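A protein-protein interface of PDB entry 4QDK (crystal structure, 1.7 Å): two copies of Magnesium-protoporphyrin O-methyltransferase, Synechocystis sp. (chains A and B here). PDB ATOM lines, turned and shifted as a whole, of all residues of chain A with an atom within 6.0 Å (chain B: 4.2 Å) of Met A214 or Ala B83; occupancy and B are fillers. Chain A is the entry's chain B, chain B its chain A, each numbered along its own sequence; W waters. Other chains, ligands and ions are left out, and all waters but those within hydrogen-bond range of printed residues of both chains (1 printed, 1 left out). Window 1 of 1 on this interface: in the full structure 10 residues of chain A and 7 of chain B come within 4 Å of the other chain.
O of Gln B82 sits at hydrogen-bond distance from NH1 of Arg A223 (3.4 Å). The side-chain amide oxygen of Gln B82 sits close to the side-chain hydroxyl of Thr A212, at 3.5 Å. The backbone NH of Met A214 sits at hydrogen-bond distance from the backbone carbonyl oxygen of Gln B82.
SD of Met A214 sits close to N of Arg A223 (3.8 Å). OE1 of Glu A195 is in salt-bridge range of NE of Arg A223 (2.8 Å). The backbone NH (N) of Gly A213 lies within hydrogen-bond range of the backbone carbonyl oxygen (O) of Ile A224 (2.9 Å). The backbone carbonyl oxygen of Phe A164 sits at hydrogen-bond distance from the backbone NH of Arg A223 (2.8 Å). The side-chain hydroxyl (OG1) of Thr A212 lies within hydrogen-bond range of the guanidinium group (NH1) of Arg A223, at 3.2 Å. The guanidinium group (NH1) of Arg A223 lies within hydrogen-bond range of the backbone carbonyl oxygen (O) of Gly A213, 2.9 Å away.
Among the printed residues, pairs that only touch across the chains: Gly A213 with Gln B82, Arg A223 with Ala B83, Met A214 with Ala B83 and Ser A216 with Pro B62.
Phe A164 touches none of the printed residues of chain B. Glu A195 touches none of the printed residues of chain B. Printed residues of chain B within 4 Å of Thr A212: Gln B82 (3.1 Å). Of the printed residues of chain B, Gly A213 touches Gln B82. Of chain B, only Gln B82 and Ala B83 come within 4 Å of Met A214. Printed residues of chain B within 4 Å of Ser A216: Pro B62. Printed residues of chain A within 4 Å of Pro B62: Ser A216 (3.96 Å). Printed residues of chain A within 4 Å of Gln B82: Thr A212 (3.1 Å), Gly A213 (3.3 Å), Met A214 (3.3 Å) and Arg A223 (3.4 Å). Of chain A, only Met A214 and Arg A223 come within 4 Å of Ala B83. The nearest printed residue of chain B that does not touch Met A214 is Pro B62 (4.3 Å). The nearest residue of chain A that does not touch Ala B83 is Thr A212 (4.6 Å).
Of the 9 printed residues of chain B, 3 touch a printed residue of chain A. Of the 13 printed residues of chain A, 5 touch a printed residue of chain B. Printed residues of chain A that touch a printed residue of chain B: Thr A212, Gly A213, Met A214, Ser A216 and Arg A223. Hydrophobic or aromatic side chains of chain A within 4 Å of the printed part of chain B: Met A214.
No position is printed for both chains.
Water W1 lies within hydrogen-bond range of the guanidinium group (NH2) of Arg A223 (2.7 Å), the side-chain hydroxyl (OG1) of Thr A212 (2.8 Å) and the backbone carbonyl oxygen (O) of Pro B79 (2.9 Å).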
ATOM      1  N   PHE A 164       5.048 -26.711  27.538  1.00  0.00           N
ATOM      2  CA  PHE A 164       6.143 -27.665  27.595  1.00  0.00           C
ATOM      3  C   PHE A 164       6.788 -27.792  26.225  1.00  0.00           C
ATOM      4  O   PHE A 164       6.155 -27.525  25.205  1.00  0.00           O
ATOM      5  CB  PHE A 164       5.636 -29.031  28.069  1.00  0.00           C
ATOM      6  CG  PHE A 164       4.578 -29.633  27.180  1.00  0.00           C
ATOM      7  CD1 PHE A 164       3.241 -29.300  27.347  1.00  0.00           C
ATOM      8  CD2 PHE A 164       4.920 -30.533  26.182  1.00  0.00           C
ATOM      9  CE1 PHE A 164       2.265 -29.849  26.533  1.00  0.00           C
ATOM     10  CE2 PHE A 164       3.948 -31.086  25.365  1.00  0.00           C
ATOM     11  CZ  PHE A 164       2.619 -30.744  25.541  1.00  0.00           C
ATOM     12  N   PRO A 166       7.666 -29.925  23.333  1.00  0.00           N
ATOM     13  CA  PRO A 166       7.196 -31.217  22.837  1.00  0.00           C
ATOM     14  C   PRO A 166       8.255 -31.883  21.982  1.00  0.00           C
ATOM     15  O   PRO A 166       9.289 -31.278  21.693  1.00  0.00           O
ATOM     16  CB  PRO A 166       6.023 -30.819  21.951  1.00  0.00           C
ATOM     17  CG  PRO A 166       6.454 -29.507  21.372  1.00  0.00           C
ATOM     18  CD  PRO A 166       7.250 -28.814  22.458  1.00  0.00           C
ATOM     19  N   THR A 168       9.527 -32.268  18.757  1.00  0.00           N
ATOM     20  CA  THR A 168       9.346 -31.444  17.572  1.00  0.00           C
ATOM     21  C   THR A 168      10.590 -31.494  16.687  1.00  0.00           C
ATOM     22  O   THR A 168      11.708 -31.665  17.180  1.00  0.00           O
ATOM     23  CB  THR A 168       8.974 -29.987  17.947  1.00  0.00           C
ATOM     24  OG1 THR A 168       8.405 -29.324  16.811  1.00  0.00           O
ATOM     25  CG2 THR A 168      10.191 -29.221  18.440  1.00  0.00           C
ATOM     26  N   GLU A 195       2.993 -34.881  23.945  1.00  0.00           N
ATOM     27  CA  GLU A 195       1.669 -34.309  24.155  1.00  0.00           C
ATOM     28  C   GLU A 195       0.670 -35.377  24.597  1.00  0.00           C
ATOM     29  O   GLU A 195      -0.191 -35.117  25.439  1.00  0.00           O
ATOM     30  CB  GLU A 195       1.174 -33.596  22.895  1.00  0.00           C
ATOM     31  CG  GLU A 195      -0.253 -33.087  23.006  1.00  0.00           C
ATOM     32  CD  GLU A 195      -0.607 -32.072  21.939  1.00  0.00           C
ATOM     33  OE1 GLU A 195       0.320 -31.481  21.343  1.00  0.00           O
ATOM     34  OE2 GLU A 195      -1.814 -31.863  21.701  1.00  0.00           O
ATOM     35  N   THR A 212      -5.529 -24.654  22.368  1.00  0.00           N
ATOM     36  CA  THR A 212      -4.107 -24.987  22.371  1.00  0.00           C
ATOM     37  C   THR A 212      -3.339 -23.971  21.543  1.00  0.00           C
ATOM     38  O   THR A 212      -3.918 -23.226  20.750  1.00  0.00           O
ATOM     39  CB  THR A 212      -3.810 -26.395  21.801  1.00  0.00           C
ATOM     40  OG1 THR A 212      -4.040 -26.409  20.387  1.00  0.00           O
ATOM     41  CG2 THR A 212      -4.670 -27.456  22.470  1.00  0.00           C
ATOM     42  N   GLY A 213      -2.027 -23.948  21.737  1.00  0.00           N
ATOM     43  CA  GLY A 213      -1.161 -23.082  20.967  1.00  0.00           C
ATOM     44  C   GLY A 213       0.196 -23.724  20.793  1.00  0.00           C
ATOM     45  O   GLY A 213       0.485 -24.767  21.383  1.00  0.00           O
ATOM     46  N   MET A 214       1.034 -23.103  19.973  1.00  0.00           N
ATOM     47  CA  MET A 214       2.377 -23.606  19.742  1.00  0.00           C
ATOM     48  C   MET A 214       3.298 -22.469  19.338  1.00  0.00           C
ATOM     49  O   MET A 214       3.100 -21.837  18.300  1.00  0.00           O
ATOM     50  CB  MET A 214       2.369 -24.679  18.651  1.00  0.00           C
ATOM     51  CG  MET A 214       3.746 -25.220  18.305  1.00  0.00           C
ATOM     52  SD  MET A 214       4.497 -26.155  19.652  1.00  0.00           S
ATOM     53  CE  MET A 214       6.166 -26.359  19.030  1.00  0.00           C
ATOM     54  N   THR A 215       4.300 -22.204  20.165  1.00  0.00           N
ATOM     55  CA  THR A 215       5.298 -21.194  19.840  1.00  0.00           C
ATOM     56  C   THR A 215       6.532 -21.856  19.237  1.00  0.00           C
ATOM     57  O   THR A 215       7.142 -22.725  19.857  1.00  0.00           O
ATOM     58  CB  THR A 215       5.719 -20.385  21.077  1.00  0.00           C
ATOM     59  OG1 THR A 215       4.560 -19.804  21.694  1.00  0.00           O
ATOM     60  CG2 THR A 215       6.683 -19.280  20.680  1.00  0.00           C
ATOM     61  N   SER A 216       6.889 -21.448  18.024  1.00  0.00           N
ATOM     62  CA  SER A 216       8.059 -21.994  17.350  1.00  0.00           C
ATOM     63  C   SER A 216       8.936 -20.885  16.793  1.00  0.00           C
ATOM     64  O   SER A 216       8.558 -20.206  15.837  1.00  0.00           O
ATOM     65  CB  SER A 216       7.646 -22.924  16.206  1.00  0.00           C
ATOM     66  OG  SER A 216       6.930 -24.049  16.681  1.00  0.00           O
ATOM     67  N   TYR A 221      10.796 -23.621  21.539  1.00  0.00           N
ATOM     68  CA  TYR A 221       9.637 -24.406  21.136  1.00  0.00           C
ATOM     69  C   TYR A 221       8.772 -24.709  22.352  1.00  0.00           C
ATOM     70  O   TYR A 221       9.199 -25.417  23.265  1.00  0.00           O
ATOM     71  CB  TYR A 221      10.078 -25.713  20.468  1.00  0.00           C
ATOM     72  CG  TYR A 221      10.971 -25.521  19.264  1.00  0.00           C
ATOM     73  CD1 TYR A 221      10.435 -25.418  17.986  1.00  0.00           C
ATOM     74  CD2 TYR A 221      12.350 -25.442  19.403  1.00  0.00           C
ATOM     75  CE1 TYR A 221      11.249 -25.241  16.882  1.00  0.00           C
ATOM     76  CE2 TYR A 221      13.171 -25.264  18.307  1.00  0.00           C
ATOM     77  CZ  TYR A 221      12.615 -25.165  17.049  1.00  0.00           C
ATOM     78  OH  TYR A 221      13.431 -24.988  15.955  1.00  0.00           O
ATOM     79  N   SER A 222       7.558 -24.174  22.363  1.00  0.00           N
ATOM     80  CA  SER A 222       6.679 -24.345  23.513  1.00  0.00           C
ATOM     81  C   SER A 222       5.243 -24.646  23.099  1.00  0.00           C
ATOM     82  O   SER A 222       4.568 -23.810  22.494  1.00  0.00           O
ATOM     83  CB  SER A 222       6.731 -23.108  24.415  1.00  0.00           C
ATOM     84  OG  SER A 222       6.043 -23.331  25.636  1.00  0.00           O
ATOM     85  N   ARG A 223       4.793 -25.853  23.425  1.00  0.00           N
ATOM     86  CA  ARG A 223       3.418 -26.269  23.187  1.00  0.00           C
ATOM     87  C   ARG A 223       2.573 -25.835  24.378  1.00  0.00           C
ATOM     88  O   ARG A 223       2.944 -26.078  25.523  1.00  0.00           O
ATOM     89  CB  ARG A 223       3.357 -27.790  23.018  1.00  0.00           C
ATOM     90  CG  ARG A 223       1.964 -28.362  22.782  1.00  0.00           C
ATOM     91  CD  ARG A 223       1.384 -27.892  21.460  1.00  0.00           C
ATOM     92  NE  ARG A 223       0.260 -28.723  21.044  1.00  0.00           N
ATOM     93  CZ  ARG A 223      -0.802 -28.272  20.385  1.00  0.00           C
ATOM     94  NH1 ARG A 223      -0.892 -26.985  20.065  1.00  0.00           N
ATOM     95  NH2 ARG A 223      -1.776 -29.107  20.052  1.00  0.00           N
ATOM     96  N   ILE A 224       1.448 -25.184  24.107  1.00  0.00           N
ATOM     97  CA  ILE A 224       0.596 -24.651  25.164  1.00  0.00           C
ATOM     98  C   ILE A 224      -0.768 -25.334  25.160  1.00  0.00           C
ATOM     99  O   ILE A 224      -1.442 -25.377  24.133  1.00  0.00           O
ATOM    100  CB  ILE A 224       0.390 -23.133  24.989  1.00  0.00           C
ATOM    101  CG1 ILE A 224       1.720 -22.453  24.657  1.00  0.00           C
ATOM    102  CG2 ILE A 224      -0.231 -22.533  26.239  1.00  0.00           C
ATOM    103  CD1 ILE A 224       1.566 -21.060  24.091  1.00  0.00           C
ATOM    104  N   LEU B  61       4.583 -31.273  12.599  1.00  0.00           N
ATOM    105  CA  LEU B  61       3.367 -30.527  12.287  1.00  0.00           C
ATOM    106  C   LEU B  61       3.566 -29.004  12.150  1.00  0.00           C
ATOM    107  O   LEU B  61       2.985 -28.395  11.250  1.00  0.00           O
ATOM    108  CB  LEU B  61       2.246 -30.856  13.280  1.00  0.00           C
ATOM    109  CG  LEU B  61       0.844 -30.378  12.890  1.00  0.00           C
ATOM    110  CD1 LEU B  61       0.461 -30.884  11.499  1.00  0.00           C
ATOM    111  CD2 LEU B  61      -0.169 -30.832  13.924  1.00  0.00           C
ATOM    112  N   PRO B  62       4.370 -28.378  13.034  1.00  0.00           N
ATOM    113  CA  PRO B  62       4.582 -26.940  12.830  1.00  0.00           C
ATOM    114  C   PRO B  62       5.221 -26.630  11.478  1.00  0.00           C
ATOM    115  O   PRO B  62       6.316 -27.109  11.188  1.00  0.00           O
ATOM    116  CB  PRO B  62       5.544 -26.567  13.961  1.00  0.00           C
ATOM    117  CG  PRO B  62       5.253 -27.550  15.029  1.00  0.00           C
ATOM    118  CD  PRO B  62       4.944 -28.832  14.315  1.00  0.00           C
ATOM    119  N   PRO B  79      -7.786 -26.948  15.171  1.00  0.00           N
ATOM    120  CA  PRO B  79      -6.766 -27.502  16.071  1.00  0.00           C
ATOM    121  C   PRO B  79      -5.438 -27.815  15.383  1.00  0.00           C
ATOM    122  O   PRO B  79      -4.400 -27.799  16.044  1.00  0.00           O
ATOM    123  CB  PRO B  79      -7.415 -28.792  16.580  1.00  0.00           C
ATOM    124  CG  PRO B  79      -8.415 -29.144  15.550  1.00  0.00           C
ATOM    125  CD  PRO B  79      -8.957 -27.833  15.083  1.00  0.00           C
ATOM    126  N   LEU B  80      -5.464 -28.094  14.084  1.00  0.00           N
ATOM    127  CA  LEU B  80      -4.218 -28.297  13.349  1.00  0.00           C
ATOM    128  C   LEU B  80      -3.436 -26.991  13.282  1.00  0.00           C
ATOM    129  O   LEU B  80      -2.215 -26.974  13.453  1.00  0.00           O
ATOM    130  CB  LEU B  80      -4.481 -28.835  11.941  1.00  0.00           C
ATOM    131  CG  LEU B  80      -4.901 -30.305  11.847  1.00  0.00           C
ATOM    132  CD1 LEU B  80      -4.967 -30.764  10.400  1.00  0.00           C
ATOM    133  CD2 LEU B  80      -3.951 -31.178  12.651  1.00  0.00           C
ATOM    134  N   ALA B  81      -4.148 -25.896  13.045  1.00  0.00           N
ATOM    135  CA  ALA B  81      -3.520 -24.581  12.978  1.00  0.00           C
ATOM    136  C   ALA B  81      -3.012 -24.154  14.347  1.00  0.00           C
ATOM    137  O   ALA B  81      -1.962 -23.516  14.457  1.00  0.00           O
ATOM    138  CB  ALA B  81      -4.488 -23.554  12.421  1.00  0.00           C
ATOM    139  N   GLN B  82      -3.751 -24.526  15.389  1.00  0.00           N
ATOM    140  CA  GLN B  82      -3.346 -24.246  16.763  1.00  0.00           C
ATOM    141  C   GLN B  82      -2.013 -24.909  17.078  1.00  0.00           C
ATOM    142  O   GLN B  82      -1.222 -24.399  17.874  1.00  0.00           O
ATOM    143  CB  GLN B  82      -4.412 -24.739  17.748  1.00  0.00           C
ATOM    144  CG  GLN B  82      -5.657 -23.878  17.799  1.00  0.00           C
ATOM    145  CD  GLN B  82      -6.731 -24.431  18.715  1.00  0.00           C
ATOM    146  OE1 GLN B  82      -6.996 -25.634  18.729  1.00  0.00           O
ATOM    147  NE2 GLN B  82      -7.358 -23.551  19.488  1.00  0.00           N
ATOM    148  N   ALA B  83      -1.775 -26.051  16.443  1.00  0.00           N
ATOM    149  CA  ALA B  83      -0.558 -26.819  16.660  1.00  0.00           C
ATOM    150  C   ALA B  83       0.555 -26.400  15.700  1.00  0.00           C
ATOM    151  O   ALA B  83       1.643 -26.975  15.717  1.00  0.00           O
ATOM    152  CB  ALA B  83      -0.847 -28.312  16.535  1.00  0.00           C
ATOM    153  N   GLY B  84       0.277 -25.400  14.867  1.00  0.00           N
ATOM    154  CA  GLY B  84       1.293 -24.807  14.013  1.00  0.00           C
ATOM    155  C   GLY B  84       1.253 -25.177  12.540  1.00  0.00           C
ATOM    156  O   GLY B  84       2.106 -24.741  11.762  1.00  0.00           O
ATOM    157  N   ALA B  85       0.270 -25.979  12.144  1.00  0.00           N
ATOM    158  CA  ALA B  85       0.169 -26.412  10.755  1.00  0.00           C
ATOM    159  C   ALA B  85      -0.249 -25.267   9.838  1.00  0.00           C
ATOM    160  O   ALA B  85      -0.908 -24.319  10.267  1.00  0.00           O
ATOM    161  CB  ALA B  85      -0.804 -27.576  10.625  1.00  0.00           C
HETATM  162  O   HOH W   1      -4.131 -28.716  18.732  1.00  0.00           O
